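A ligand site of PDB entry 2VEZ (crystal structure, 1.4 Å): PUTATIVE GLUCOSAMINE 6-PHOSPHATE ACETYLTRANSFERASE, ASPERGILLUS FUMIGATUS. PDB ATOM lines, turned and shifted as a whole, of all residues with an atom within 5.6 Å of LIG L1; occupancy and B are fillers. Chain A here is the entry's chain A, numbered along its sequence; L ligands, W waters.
An oxygen (O4) of LIG L1 lies within salt-bridge range of the side-chain amino group of Lys 176 (2.8 Å). The backbone NH of Leu 144 is in hydrogen-bond range of an oxygen (O9) of LIG L1, at 2.8 Å. The backbone NH (N) of Lys 141 sits at hydrogen-bond distance from an oxygen (O8) of LIG L1, 2.8 Å away. O5 of LIG L1 is in salt-bridge range of NZ of Lys 141 (3.2 Å). The backbone NH (N) of Ile 131 sits at hydrogen-bond distance from an oxygen (O17) of LIG L1, at 3.0 Å. O of Ile 131 lies within hydrogen-bond range of N7 of LIG L1 (2.8 Å). O15 of LIG L1 lies within hydrogen-bond range of N of Val 133, 2.9 Å away. The backbone NH of Gly 143 is in hydrogen-bond range of an oxygen (O12) of LIG L1 (2.9 Å). O of Ala 169 lies within hydrogen-bond range of N3 of LIG L1 (3.0 Å). An oxygen (O11) of LIG L1 is in hydrogen-bond range of the backbone NH (N) of Gly 139, at 3.2 Å. The side-chain hydroxyl of Tyr 174 lies close to a sulfur (S1) of LIG L1 (3.2 Å). N of Lys 140 sits at hydrogen-bond distance from O8 of LIG L1 (3.3 Å). OD1 of Asn 170 lies close to O16 of LIG L1, at 3.3 Å. The side-chain amide oxygen (OE1) of Gln 138 lies close to an oxygen (O14) of LIG L1, 3.5 Å away. An oxygen (O17) of LIG L1 lies within hydrogen-bond range of the backbone NH of Asp 130. The backbone NH (N) of Asp 130 sits at hydrogen-bond distance from an oxygen (O3) of LG2 L2 (2.9 Å). The side-chain carboxylate (OD1) of Asp 130 lies within hydrogen-bond range of an oxygen (O4) of LG2 L2, 2.7 Å away. The backbone carbonyl oxygen (O) of Asp 165 sits at hydrogen-bond distance from an oxygen (O2) of LG2 L2. An oxygen (O3) of LG2 L2 lies within hydrogen-bond range of the side-chain carboxylate of Glu 129 (2.9 Å).
S1 of LIG L1 sits close to O1 of LG2 L2.
The backbone carbonyl oxygen (O) of Val 133 is in hydrogen-bond range of the side-chain amide nitrogen (NE2) of Gln 138 (2.9 Å). ND2 of Asn 170 lies close to SG of Cys 166.
O of Asp 165 sits close to S1 of LIG L1. Merely in contact with LIG L1: Phe 173, Ala 132, Leu 69, Leu 142, Gly 172, Val 68 and Ile 128. Hydrophobic or aromatic side chains that line LIG L1: Val 68, Leu 69, Ile 131, Val 133, Leu 144, Phe 173 and Tyr 174. Of the 28 residues printed, 21 come within 4 Å of LIG L1.
Water W11 lies within hydrogen-bond range of N1 of LIG L1 (2.7 Å) and O of Ala 169 (2.8 Å). Water W3 lies within hydrogen-bond range of O11 of LIG L1 and N of Gly 139. Water W2 lies within hydrogen-bond range of an oxygen (O8) of LIG L1 (2.8 Å), the side-chain amino group of Lys 141 (3.0 Å) and the backbone carbonyl oxygen of Gly 139 (3.1 Å). Water W12 lies within hydrogen-bond range of the side-chain amino group of Lys 176 and a nitrogen (N2) of LIG L1. Water W6 lies within hydrogen-bond range of N6 of LIG L1 (3.1 Å) and OE1 of Gln 138 (3.3 Å). Water W5 lies within hydrogen-bond range of the side-chain amide oxygen of Asn 170 (2.8 Å), an oxygen (O1) of LG2 L2 (3.1 Å) and a sulfur (S1) of LIG L1 (3.3 Å).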
ATOM      1  N   VAL A  68      -5.171  16.299   7.090  1.00  0.00           N
ATOM      2  CA  VAL A  68      -6.426  15.568   6.980  1.00  0.00           C
ATOM      3  C   VAL A  68      -6.660  15.046   5.559  1.00  0.00           C
ATOM      4  O   VAL A  68      -7.415  14.113   5.342  1.00  0.00           O
ATOM      5  CB  VAL A  68      -7.672  16.365   7.457  1.00  0.00           C
ATOM      6  CG1 VAL A  68      -7.430  16.982   8.828  1.00  0.00           C
ATOM      7  CG2 VAL A  68      -8.070  17.403   6.458  1.00  0.00           C
ATOM      8  N   LEU A  69      -6.006  15.657   4.581  1.00  0.00           N
ATOM      9  CA  LEU A  69      -6.334  15.357   3.192  1.00  0.00           C
ATOM     10  C   LEU A  69      -5.508  14.185   2.756  1.00  0.00           C
ATOM     11  O   LEU A  69      -6.030  13.199   2.208  1.00  0.00           O
ATOM     12  CB  LEU A  69      -6.072  16.580   2.283  1.00  0.00           C
ATOM     13  CG  LEU A  69      -6.923  16.814   1.021  1.00  0.00           C
ATOM     14  CD1 LEU A  69      -6.069  17.592   0.011  1.00  0.00           C
ATOM     15  CD2 LEU A  69      -7.579  15.587   0.357  1.00  0.00           C
ATOM     16  N   ILE A 128     -10.222  23.416  -8.645  1.00  0.00           N
ATOM     17  CA  ILE A 128     -10.223  23.466  -7.179  1.00  0.00           C
ATOM     18  C   ILE A 128      -9.391  22.289  -6.658  1.00  0.00           C
ATOM     19  O   ILE A 128      -9.514  21.156  -7.136  1.00  0.00           O
ATOM     20  CB  ILE A 128     -11.659  23.486  -6.627  1.00  0.00           C
ATOM     21  CG1 ILE A 128     -12.235  24.900  -6.783  1.00  0.00           C
ATOM     22  CG2 ILE A 128     -11.695  22.976  -5.160  1.00  0.00           C
ATOM     23  CD1 ILE A 128     -13.697  25.023  -6.375  1.00  0.00           C
ATOM     24  N   GLU A 129      -8.491  22.585  -5.723  1.00  0.00           N
ATOM     25  CA  GLU A 129      -7.517  21.629  -5.218  1.00  0.00           C
ATOM     26  C   GLU A 129      -7.354  21.726  -3.709  1.00  0.00           C
ATOM     27  O   GLU A 129      -7.501  22.804  -3.108  1.00  0.00           O
ATOM     28  CB  GLU A 129      -6.116  21.907  -5.796  1.00  0.00           C
ATOM     29  CG  GLU A 129      -6.039  21.959  -7.308  1.00  0.00           C
ATOM     30  CD  GLU A 129      -6.149  20.593  -7.976  1.00  0.00           C
ATOM     31  OE1 GLU A 129      -6.032  19.533  -7.299  1.00  0.00           O
ATOM     32  OE2 GLU A 129      -6.304  20.596  -9.228  1.00  0.00           O
ATOM     33  N   ASP A 130      -7.011  20.590  -3.111  1.00  0.00           N
ATOM     34  CA  ASP A 130      -6.475  20.592  -1.759  1.00  0.00           C
ATOM     35  C   ASP A 130      -7.371  21.266  -0.730  1.00  0.00           C
ATOM     36  O   ASP A 130      -6.929  22.131   0.053  1.00  0.00           O
ATOM     37  CB  ASP A 130      -5.055  21.180  -1.753  1.00  0.00           C
ATOM     38  CG  ASP A 130      -4.116  20.411  -2.684  1.00  0.00           C
ATOM     39  OD1 ASP A 130      -4.386  19.220  -2.885  1.00  0.00           O
ATOM     40  OD2 ASP A 130      -3.130  20.999  -3.193  1.00  0.00           O
ATOM     41  N   ILE A 131      -8.623  20.800  -0.713  1.00  0.00           N
ATOM     42  CA  ILE A 131      -9.648  21.282   0.206  1.00  0.00           C
ATOM     43  C   ILE A 131      -9.563  20.456   1.480  1.00  0.00           C
ATOM     44  O   ILE A 131      -9.634  19.237   1.426  1.00  0.00           O
ATOM     45  CB  ILE A 131     -11.055  21.094  -0.413  1.00  0.00           C
ATOM     46  CG1 ILE A 131     -11.127  21.778  -1.778  1.00  0.00           C
ATOM     47  CG2 ILE A 131     -12.155  21.630   0.516  1.00  0.00           C
ATOM     48  CD1 ILE A 131     -10.829  23.288  -1.764  1.00  0.00           C
ATOM     49  N   ALA A 132      -9.411  21.132   2.623  1.00  0.00           N
ATOM     50  CA  ALA A 132      -9.219  20.424   3.885  1.00  0.00           C
ATOM     51  C   ALA A 132      -9.760  21.250   5.036  1.00  0.00           C
ATOM     52  O   ALA A 132      -9.513  22.448   5.108  1.00  0.00           O
ATOM     53  CB  ALA A 132      -7.745  20.110   4.097  1.00  0.00           C
ATOM     54  N   VAL A 133     -10.456  20.591   5.955  1.00  0.00           N
ATOM     55  CA  VAL A 133     -10.900  21.255   7.177  1.00  0.00           C
ATOM     56  C   VAL A 133     -10.468  20.380   8.362  1.00  0.00           C
ATOM     57  O   VAL A 133     -10.696  19.157   8.353  1.00  0.00           O
ATOM     58  CB  VAL A 133     -12.440  21.459   7.146  1.00  0.00           C
ATOM     59  CG1 VAL A 133     -12.962  21.975   8.472  1.00  0.00           C
ATOM     60  CG2 VAL A 133     -12.845  22.413   6.051  1.00  0.00           C
ATOM     61  N   GLU A 134      -9.850  20.988   9.367  1.00  0.00           N
ATOM     62  CA  GLU A 134      -9.455  20.284  10.591  1.00  0.00           C
ATOM     63  C   GLU A 134     -10.616  19.435  11.099  1.00  0.00           C
ATOM     64  O   GLU A 134     -11.753  19.914  11.101  1.00  0.00           O
ATOM     65  CB  GLU A 134      -9.110  21.366  11.607  1.00  0.00           C
ATOM     66  CG  GLU A 134      -8.748  21.002  12.982  1.00  0.00           C
ATOM     67  CD  GLU A 134      -8.377  22.262  13.714  1.00  0.00           C
ATOM     68  OE1 GLU A 134      -7.296  22.786  13.419  1.00  0.00           O
ATOM     69  OE2 GLU A 134      -9.223  22.758  14.488  1.00  0.00           O
ATOM     70  N   GLN A 137     -13.292  20.863  13.335  1.00  0.00           N
ATOM     71  CA  GLN A 137     -14.000  22.004  12.750  1.00  0.00           C
ATOM     72  C   GLN A 137     -14.873  21.579  11.565  1.00  0.00           C
ATOM     73  O   GLN A 137     -15.519  22.404  10.942  1.00  0.00           O
ATOM     74  CB  GLN A 137     -13.012  23.098  12.345  1.00  0.00           C
ATOM     75  CG  GLN A 137     -12.183  23.602  13.524  1.00  0.00           C
ATOM     76  CD  GLN A 137     -12.866  24.693  14.317  1.00  0.00           C
ATOM     77  OE1 GLN A 137     -13.949  25.145  13.982  1.00  0.00           O
ATOM     78  NE2 GLN A 137     -12.220  25.110  15.399  1.00  0.00           N
ATOM     79  N   GLN A 138     -14.903  20.286  11.276  1.00  0.00           N
ATOM     80  CA  GLN A 138     -15.748  19.779  10.196  1.00  0.00           C
ATOM     81  C   GLN A 138     -17.244  19.816  10.515  1.00  0.00           C
ATOM     82  O   GLN A 138     -17.645  19.859  11.685  1.00  0.00           O
ATOM     83  CB  GLN A 138     -15.310  18.354   9.810  1.00  0.00           C
ATOM     84  CG  GLN A 138     -14.009  18.329   9.065  1.00  0.00           C
ATOM     85  CD  GLN A 138     -13.561  16.901   8.740  1.00  0.00           C
ATOM     86  OE1 GLN A 138     -14.338  15.942   8.884  1.00  0.00           O
ATOM     87  NE2 GLN A 138     -12.305  16.757   8.304  1.00  0.00           N
ATOM     88  N   GLY A 139     -18.057  19.848   9.472  1.00  0.00           N
ATOM     89  CA  GLY A 139     -19.510  19.803   9.607  1.00  0.00           C
ATOM     90  C   GLY A 139     -20.146  21.069  10.141  1.00  0.00           C
ATOM     91  O   GLY A 139     -21.231  21.022  10.747  1.00  0.00           O
ATOM     92  N   LYS A 140     -19.486  22.205   9.912  1.00  0.00           N
ATOM     93  CA  LYS A 140     -19.953  23.527  10.352  1.00  0.00           C
ATOM     94  C   LYS A 140     -20.036  24.508   9.177  1.00  0.00           C
ATOM     95  O   LYS A 140     -20.051  25.737   9.374  1.00  0.00           O
ATOM     96  CB  LYS A 140     -18.969  24.160  11.381  1.00  0.00           C
ATOM     97  CG  LYS A 140     -18.693  23.377  12.637  1.00  0.00           C
ATOM     98  CD  LYS A 140     -17.706  24.164  13.480  1.00  0.00           C
ATOM     99  CE  LYS A 140     -17.757  23.789  14.952  1.00  0.00           C
ATOM    100  NZ  LYS A 140     -17.158  22.458  15.211  1.00  0.00           N
ATOM    101  N   LYS A 141     -20.097  23.971   7.946  1.00  0.00           N
ATOM    102  CA  LYS A 141     -20.237  24.799   6.741  1.00  0.00           C
ATOM    103  C   LYS A 141     -18.920  25.444   6.270  1.00  0.00           C
ATOM    104  O   LYS A 141     -18.918  26.152   5.278  1.00  0.00           O
ATOM    105  CB  LYS A 141     -21.343  25.878   6.843  1.00  0.00           C
ATOM    106  CG  LYS A 141     -22.727  25.415   7.332  1.00  0.00           C
ATOM    107  CD  LYS A 141     -23.403  24.471   6.352  1.00  0.00           C
ATOM    108  CE  LYS A 141     -24.793  24.025   6.824  1.00  0.00           C
ATOM    109  NZ  LYS A 141     -24.707  23.265   8.088  1.00  0.00           N
ATOM    110  N   LEU A 142     -17.814  25.183   6.967  1.00  0.00           N
ATOM    111  CA  LEU A 142     -16.539  25.804   6.547  1.00  0.00           C
ATOM    112  C   LEU A 142     -16.067  25.341   5.160  1.00  0.00           C
ATOM    113  O   LEU A 142     -15.592  26.158   4.385  1.00  0.00           O
ATOM    114  CB  LEU A 142     -15.423  25.593   7.577  1.00  0.00           C
ATOM    115  CG  LEU A 142     -15.760  26.099   8.984  1.00  0.00           C
ATOM    116  CD1 LEU A 142     -14.549  25.871   9.877  1.00  0.00           C
ATOM    117  CD2 LEU A 142     -16.152  27.592   8.976  1.00  0.00           C
ATOM    118  N   GLY A 143     -16.214  24.045   4.874  1.00  0.00           N
ATOM    119  CA  GLY A 143     -15.832  23.547   3.550  1.00  0.00           C
ATOM    120  C   GLY A 143     -16.726  24.159   2.468  1.00  0.00           C
ATOM    121  O   GLY A 143     -16.223  24.601   1.411  1.00  0.00           O
ATOM    122  N   LEU A 144     -18.027  24.232   2.726  1.00  0.00           N
ATOM    123  CA  LEU A 144     -18.937  24.888   1.803  1.00  0.00           C
ATOM    124  C   LEU A 144     -18.480  26.319   1.504  1.00  0.00           C
ATOM    125  O   LEU A 144     -18.482  26.760   0.353  1.00  0.00           O
ATOM    126  CB  LEU A 144     -20.368  24.904   2.375  1.00  0.00           C
ATOM    127  CG  LEU A 144     -21.408  25.733   1.604  1.00  0.00           C
ATOM    128  CD1 LEU A 144     -21.662  25.150   0.200  1.00  0.00           C
ATOM    129  CD2 LEU A 144     -22.686  25.836   2.398  1.00  0.00           C
ATOM    130  N   ARG A 145     -18.132  27.066   2.549  1.00  0.00           N
ATOM    131  CA  ARG A 145     -17.691  28.455   2.363  1.00  0.00           C
ATOM    132  C   ARG A 145     -16.396  28.566   1.579  1.00  0.00           C
ATOM    133  O   ARG A 145     -16.250  29.484   0.758  1.00  0.00           O
ATOM    134  CB  ARG A 145     -17.568  29.190   3.705  1.00  0.00           C
ATOM    135  CG  ARG A 145     -18.866  29.210   4.564  1.00  0.00           C
ATOM    136  CD  ARG A 145     -20.141  29.520   3.777  1.00  0.00           C
ATOM    137  NE  ARG A 145     -21.337  29.435   4.632  1.00  0.00           N
ATOM    138  CZ  ARG A 145     -22.585  29.350   4.183  1.00  0.00           C
ATOM    139  NH1 ARG A 145     -22.855  29.424   2.882  1.00  0.00           N
ATOM    140  NH2 ARG A 145     -23.582  29.279   5.066  1.00  0.00           N
ATOM    141  N   LEU A 164     -13.182  19.948 -10.372  1.00  0.00           N
ATOM    142  CA  LEU A 164     -12.365  19.318  -9.355  1.00  0.00           C
ATOM    143  C   LEU A 164     -12.584  17.795  -9.458  1.00  0.00           C
ATOM    144  O   LEU A 164     -13.529  17.326 -10.101  1.00  0.00           O
ATOM    145  CB  LEU A 164     -12.748  19.852  -7.951  1.00  0.00           C
ATOM    146  CG  LEU A 164     -14.209  19.648  -7.566  1.00  0.00           C
ATOM    147  CD1 LEU A 164     -14.461  18.308  -6.805  1.00  0.00           C
ATOM    148  CD2 LEU A 164     -14.755  20.837  -6.734  1.00  0.00           C
ATOM    149  N   ASP A 165     -11.710  17.036  -8.817  1.00  0.00           N
ATOM    150  CA  ASP A 165     -11.909  15.604  -8.646  1.00  0.00           C
ATOM    151  C   ASP A 165     -12.199  15.279  -7.200  1.00  0.00           C
ATOM    152  O   ASP A 165     -11.669  15.916  -6.290  1.00  0.00           O
ATOM    153  CB  ASP A 165     -10.662  14.861  -9.104  1.00  0.00           C
ATOM    154  CG  ASP A 165     -10.385  15.033 -10.582  1.00  0.00           C
ATOM    155  OD1 ASP A 165     -11.288  14.885 -11.417  1.00  0.00           O
ATOM    156  OD2 ASP A 165      -9.247  15.331 -10.888  1.00  0.00           O
ATOM    157  N   CYS A 166     -13.039  14.273  -7.003  1.00  0.00           N
ATOM    158  CA  CYS A 166     -13.380  13.863  -5.651  1.00  0.00           C
ATOM    159  C   CYS A 166     -13.566  12.355  -5.582  1.00  0.00           C
ATOM    160  O   CYS A 166     -13.485  11.632  -6.590  1.00  0.00           O
ATOM    161  CB  CYS A 166     -14.616  14.614  -5.153  1.00  0.00           C
ATOM    162  SG  CYS A 166     -16.164  14.106  -5.932  1.00  0.00           S
ATOM    163  N   ALA A 169     -16.930   8.828  -1.723  1.00  0.00           N
ATOM    164  CA  ALA A 169     -17.340   9.128  -0.339  1.00  0.00           C
ATOM    165  C   ALA A 169     -17.597  10.618  -0.102  1.00  0.00           C
ATOM    166  O   ALA A 169     -18.365  10.975   0.784  1.00  0.00           O
ATOM    167  CB  ALA A 169     -16.325   8.586   0.645  1.00  0.00           C
ATOM    168  N   ASN A 170     -16.948  11.496  -0.876  1.00  0.00           N
ATOM    169  CA  ASN A 170     -17.253  12.907  -0.649  1.00  0.00           C
ATOM    170  C   ASN A 170     -17.986  13.598  -1.796  1.00  0.00           C
ATOM    171  O   ASN A 170     -18.235  14.820  -1.754  1.00  0.00           O
ATOM    172  CB  ASN A 170     -16.040  13.703  -0.125  1.00  0.00           C
ATOM    173  CG  ASN A 170     -14.922  13.761  -1.130  1.00  0.00           C
ATOM    174  OD1 ASN A 170     -13.752  14.010  -0.811  1.00  0.00           O
ATOM    175  ND2 ASN A 170     -15.279  13.515  -2.374  1.00  0.00           N
ATOM    176  N   GLU A 171     -18.478  12.799  -2.765  1.00  0.00           N
ATOM    177  CA  GLU A 171     -19.295  13.386  -3.821  1.00  0.00           C
ATOM    178  C   GLU A 171     -20.475  14.186  -3.268  1.00  0.00           C
ATOM    179  O   GLU A 171     -20.819  15.236  -3.785  1.00  0.00           O
ATOM    180  CB  GLU A 171     -19.803  12.318  -4.808  1.00  0.00           C
ATOM    181  CG  GLU A 171     -20.492  12.949  -6.021  1.00  0.00           C
ATOM    182  CD  GLU A 171     -21.133  11.964  -6.966  1.00  0.00           C
ATOM    183  OE1 GLU A 171     -21.209  10.775  -6.612  1.00  0.00           O
ATOM    184  OE2 GLU A 171     -21.570  12.422  -8.060  1.00  0.00           O
ATOM    185  N   GLY A 172     -21.093  13.701  -2.184  1.00  0.00           N
ATOM    186  CA  GLY A 172     -22.278  14.358  -1.632  1.00  0.00           C
ATOM    187  C   GLY A 172     -21.980  15.744  -1.101  1.00  0.00           C
ATOM    188  O   GLY A 172     -22.851  16.639  -1.151  1.00  0.00           O
ATOM    189  N   PHE A 173     -20.761  15.930  -0.574  1.00  0.00           N
ATOM    190  CA  PHE A 173     -20.337  17.256  -0.184  1.00  0.00           C
ATOM    191  C   PHE A 173     -20.335  18.200  -1.380  1.00  0.00           C
ATOM    192  O   PHE A 173     -20.878  19.297  -1.314  1.00  0.00           O
ATOM    193  CB  PHE A 173     -18.979  17.225   0.498  1.00  0.00           C
ATOM    194  CG  PHE A 173     -18.353  18.576   0.642  1.00  0.00           C
ATOM    195  CD1 PHE A 173     -17.243  18.922  -0.113  1.00  0.00           C
ATOM    196  CD2 PHE A 173     -18.896  19.498   1.524  1.00  0.00           C
ATOM    197  CE1 PHE A 173     -16.655  20.183   0.007  1.00  0.00           C
ATOM    198  CE2 PHE A 173     -18.339  20.762   1.664  1.00  0.00           C
ATOM    199  CZ  PHE A 173     -17.216  21.123   0.908  1.00  0.00           C
ATOM    200  N   TYR A 174     -19.743  17.750  -2.494  1.00  0.00           N
ATOM    201  CA  TYR A 174     -19.667  18.601  -3.684  1.00  0.00           C
ATOM    202  C   TYR A 174     -21.033  18.857  -4.338  1.00  0.00           C
ATOM    203  O   TYR A 174     -21.267  19.944  -4.849  1.00  0.00           O
ATOM    204  CB  TYR A 174     -18.614  18.074  -4.672  1.00  0.00           C
ATOM    205  CG  TYR A 174     -17.248  18.282  -4.090  1.00  0.00           C
ATOM    206  CD1 TYR A 174     -16.518  17.223  -3.561  1.00  0.00           C
ATOM    207  CD2 TYR A 174     -16.746  19.581  -3.949  1.00  0.00           C
ATOM    208  CE1 TYR A 174     -15.281  17.429  -2.941  1.00  0.00           C
ATOM    209  CE2 TYR A 174     -15.535  19.796  -3.341  1.00  0.00           C
ATOM    210  CZ  TYR A 174     -14.802  18.744  -2.854  1.00  0.00           C
ATOM    211  OH  TYR A 174     -13.610  19.029  -2.240  1.00  0.00           O
ATOM    212  N   LYS A 176     -23.743  19.210  -2.532  1.00  0.00           N
ATOM    213  CA  LYS A 176     -24.287  20.254  -1.651  1.00  0.00           C
ATOM    214  C   LYS A 176     -23.644  21.631  -1.908  1.00  0.00           C
ATOM    215  O   LYS A 176     -24.226  22.682  -1.574  1.00  0.00           O
ATOM    216  CB  LYS A 176     -24.237  19.816  -0.176  1.00  0.00           C
ATOM    217  CG  LYS A 176     -25.255  18.670   0.113  1.00  0.00           C
ATOM    218  CD  LYS A 176     -25.649  18.561   1.583  1.00  0.00           C
ATOM    219  CE  LYS A 176     -26.844  17.596   1.839  1.00  0.00           C
ATOM    220  NZ  LYS A 176     -26.961  17.047   3.271  1.00  0.00           N
HETATM  221  N1  LIG L   1     -20.684  13.290   2.155  1.00  0.00           N
HETATM  222  C1  LIG L   1     -21.905  13.847   2.194  1.00  0.00           C
HETATM  223  N2  LIG L   1     -22.152  15.040   2.781  1.00  0.00           N
HETATM  224  C2  LIG L   1     -21.142  15.728   3.368  1.00  0.00           C
HETATM  225  C3  LIG L   1     -19.789  15.179   3.385  1.00  0.00           C
HETATM  226  C4  LIG L   1     -19.599  13.882   2.725  1.00  0.00           C
HETATM  227  N3  LIG L   1     -18.366  13.316   2.701  1.00  0.00           N
HETATM  228  N4  LIG L   1     -18.992  16.051   4.044  1.00  0.00           N
HETATM  229  C5  LIG L   1     -19.799  17.091   4.411  1.00  0.00           C
HETATM  230  N5  LIG L   1     -21.073  16.887   4.024  1.00  0.00           N
HETATM  231  C6  LIG L   1     -22.254  17.784   4.182  1.00  0.00           C
HETATM  232  C7  LIG L   1     -22.344  18.518   5.501  1.00  0.00           C
HETATM  233  O1  LIG L   1     -22.917  17.664   6.521  1.00  0.00           O
HETATM  234  C8  LIG L   1     -23.222  19.692   5.077  1.00  0.00           C
HETATM  235  O2  LIG L   1     -24.567  19.247   4.872  1.00  0.00           O
HETATM  236  P1  LIG L   1     -25.892  20.116   5.215  1.00  0.00           P
HETATM  237  O3  LIG L   1     -25.992  21.208   4.190  1.00  0.00           O
HETATM  238  O4  LIG L   1     -27.019  19.111   5.127  1.00  0.00           O
HETATM  239  O5  LIG L   1     -25.472  20.586   6.583  1.00  0.00           O
HETATM  240  C9  LIG L   1     -22.682  20.068   3.693  1.00  0.00           C
HETATM  241  O6  LIG L   1     -22.144  18.825   3.182  1.00  0.00           O
HETATM  242  C10 LIG L   1     -21.543  21.087   3.747  1.00  0.00           C
HETATM  243  O7  LIG L   1     -20.441  20.521   4.459  1.00  0.00           O
HETATM  244  P2  LIG L   1     -19.458  21.348   5.404  1.00  0.00           P
HETATM  245  O8  LIG L   1     -20.048  21.432   6.773  1.00  0.00           O
HETATM  246  O9  LIG L   1     -19.082  22.613   4.721  1.00  0.00           O
HETATM  247  O10 LIG L   1     -18.305  20.237   5.409  1.00  0.00           O
HETATM  248  P3  LIG L   1     -16.820  20.336   5.970  1.00  0.00           P
HETATM  249  O11 LIG L   1     -16.570  19.117   6.793  1.00  0.00           O
HETATM  250  O12 LIG L   1     -16.519  21.688   6.580  1.00  0.00           O
HETATM  251  O13 LIG L   1     -15.876  20.146   4.679  1.00  0.00           O
HETATM  252  C11 LIG L   1     -14.610  18.414   3.630  1.00  0.00           C
HETATM  253  C12 LIG L   1     -15.998  19.003   3.840  1.00  0.00           C
HETATM  254  C13 LIG L   1     -13.714  19.441   2.935  1.00  0.00           C
HETATM  255  C14 LIG L   1     -14.777  17.196   2.719  1.00  0.00           C
HETATM  256  C15 LIG L   1     -13.978  17.995   4.980  1.00  0.00           C
HETATM  257  O14 LIG L   1     -14.883  17.124   5.683  1.00  0.00           O
HETATM  258  C16 LIG L   1     -12.594  17.394   4.885  1.00  0.00           C
HETATM  259  O15 LIG L   1     -11.599  18.100   4.983  1.00  0.00           O
HETATM  260  N6  LIG L   1     -12.500  16.055   4.710  1.00  0.00           N
HETATM  261  C17 LIG L   1     -11.234  15.330   4.608  1.00  0.00           C
HETATM  262  C18 LIG L   1     -10.391  15.749   3.395  1.00  0.00           C
HETATM  263  C19 LIG L   1     -11.221  15.761   2.132  1.00  0.00           C
HETATM  264  O16 LIG L   1     -11.938  14.800   1.836  1.00  0.00           O
HETATM  265  N7  LIG L   1     -11.108  16.850   1.361  1.00  0.00           N
HETATM  266  C20 LIG L   1     -11.709  16.976   0.049  1.00  0.00           C
HETATM  267  C21 LIG L   1     -10.787  16.396  -1.025  1.00  0.00           C
HETATM  268  S1  LIG L   1     -11.410  16.685  -2.662  1.00  0.00           S
HETATM  269  C22 LIG L   1     -10.633  18.093  -3.165  1.00  0.00           C
HETATM  270  O17 LIG L   1      -9.734  18.634  -2.485  1.00  0.00           O
HETATM  271  C23 LIG L   1     -11.090  18.740  -4.443  1.00  0.00           C
HETATM  272  C1  LG2 L   2      -8.114  14.755  -4.784  1.00  0.00           C
HETATM  273  C2  LG2 L   2      -8.293  16.268  -4.841  1.00  0.00           C
HETATM  274  C3  LG2 L   2      -6.941  16.973  -5.069  1.00  0.00           C
HETATM  275  C4  LG2 L   2      -5.884  16.543  -4.068  1.00  0.00           C
HETATM  276  C5  LG2 L   2      -5.805  15.019  -4.080  1.00  0.00           C
HETATM  277  C6  LG2 L   2      -4.761  14.532  -3.084  1.00  0.00           C
HETATM  278  O1  LG2 L   2      -9.374  14.115  -4.551  1.00  0.00           O
HETATM  279  O2  LG2 L   2      -9.117  16.615  -5.923  1.00  0.00           O
HETATM  280  O3  LG2 L   2      -7.149  18.354  -4.949  1.00  0.00           O
HETATM  281  O4  LG2 L   2      -4.642  17.086  -4.492  1.00  0.00           O
HETATM  282  O5  LG2 L   2      -7.104  14.435  -3.762  1.00  0.00           O
HETATM  283  O6  LG2 L   2      -4.660  13.126  -3.199  1.00  0.00           O
HETATM  284  P1  LG2 L   2      -3.218  12.473  -3.572  1.00  0.00           P
HETATM  285  O7  LG2 L   2      -3.376  10.904  -3.732  1.00  0.00           O
HETATM  286  O8  LG2 L   2      -2.313  12.626  -2.262  1.00  0.00           O
HETATM  287  O9  LG2 L   2      -2.502  13.134  -4.708  1.00  0.00           O
HETATM  288  O   HOH W   1     -16.626  14.865   4.883  1.00  0.00           O
HETATM  289  O   HOH W   2     -22.572  21.230   7.905  1.00  0.00           O
HETATM  290  O   HOH W   3     -18.511  17.286   7.452  1.00  0.00           O
HETATM  291  O   HOH W   4     -24.738  23.125   2.945  1.00  0.00           O
HETATM  292  O   HOH W   5     -11.589  13.368  -2.460  1.00  0.00           O
HETATM  293  O   HOH W   6     -14.264  13.963   6.245  1.00  0.00           O
HETATM  294  O   HOH W   7     -17.078  22.942   8.787  1.00  0.00           O
HETATM  295  O   HOH W   8     -15.606  12.847   3.754  1.00  0.00           O
HETATM  296  O   HOH W   9     -11.664  13.849   7.678  1.00  0.00           O
HETATM  297  O   HOH W  10     -13.110  12.454   2.617  1.00  0.00           O
HETATM  298  O   HOH W  11     -21.162  11.113   0.691  1.00  0.00           O
HETATM  299  O   HOH W  12     -24.982  15.247   2.539  1.00  0.00           O
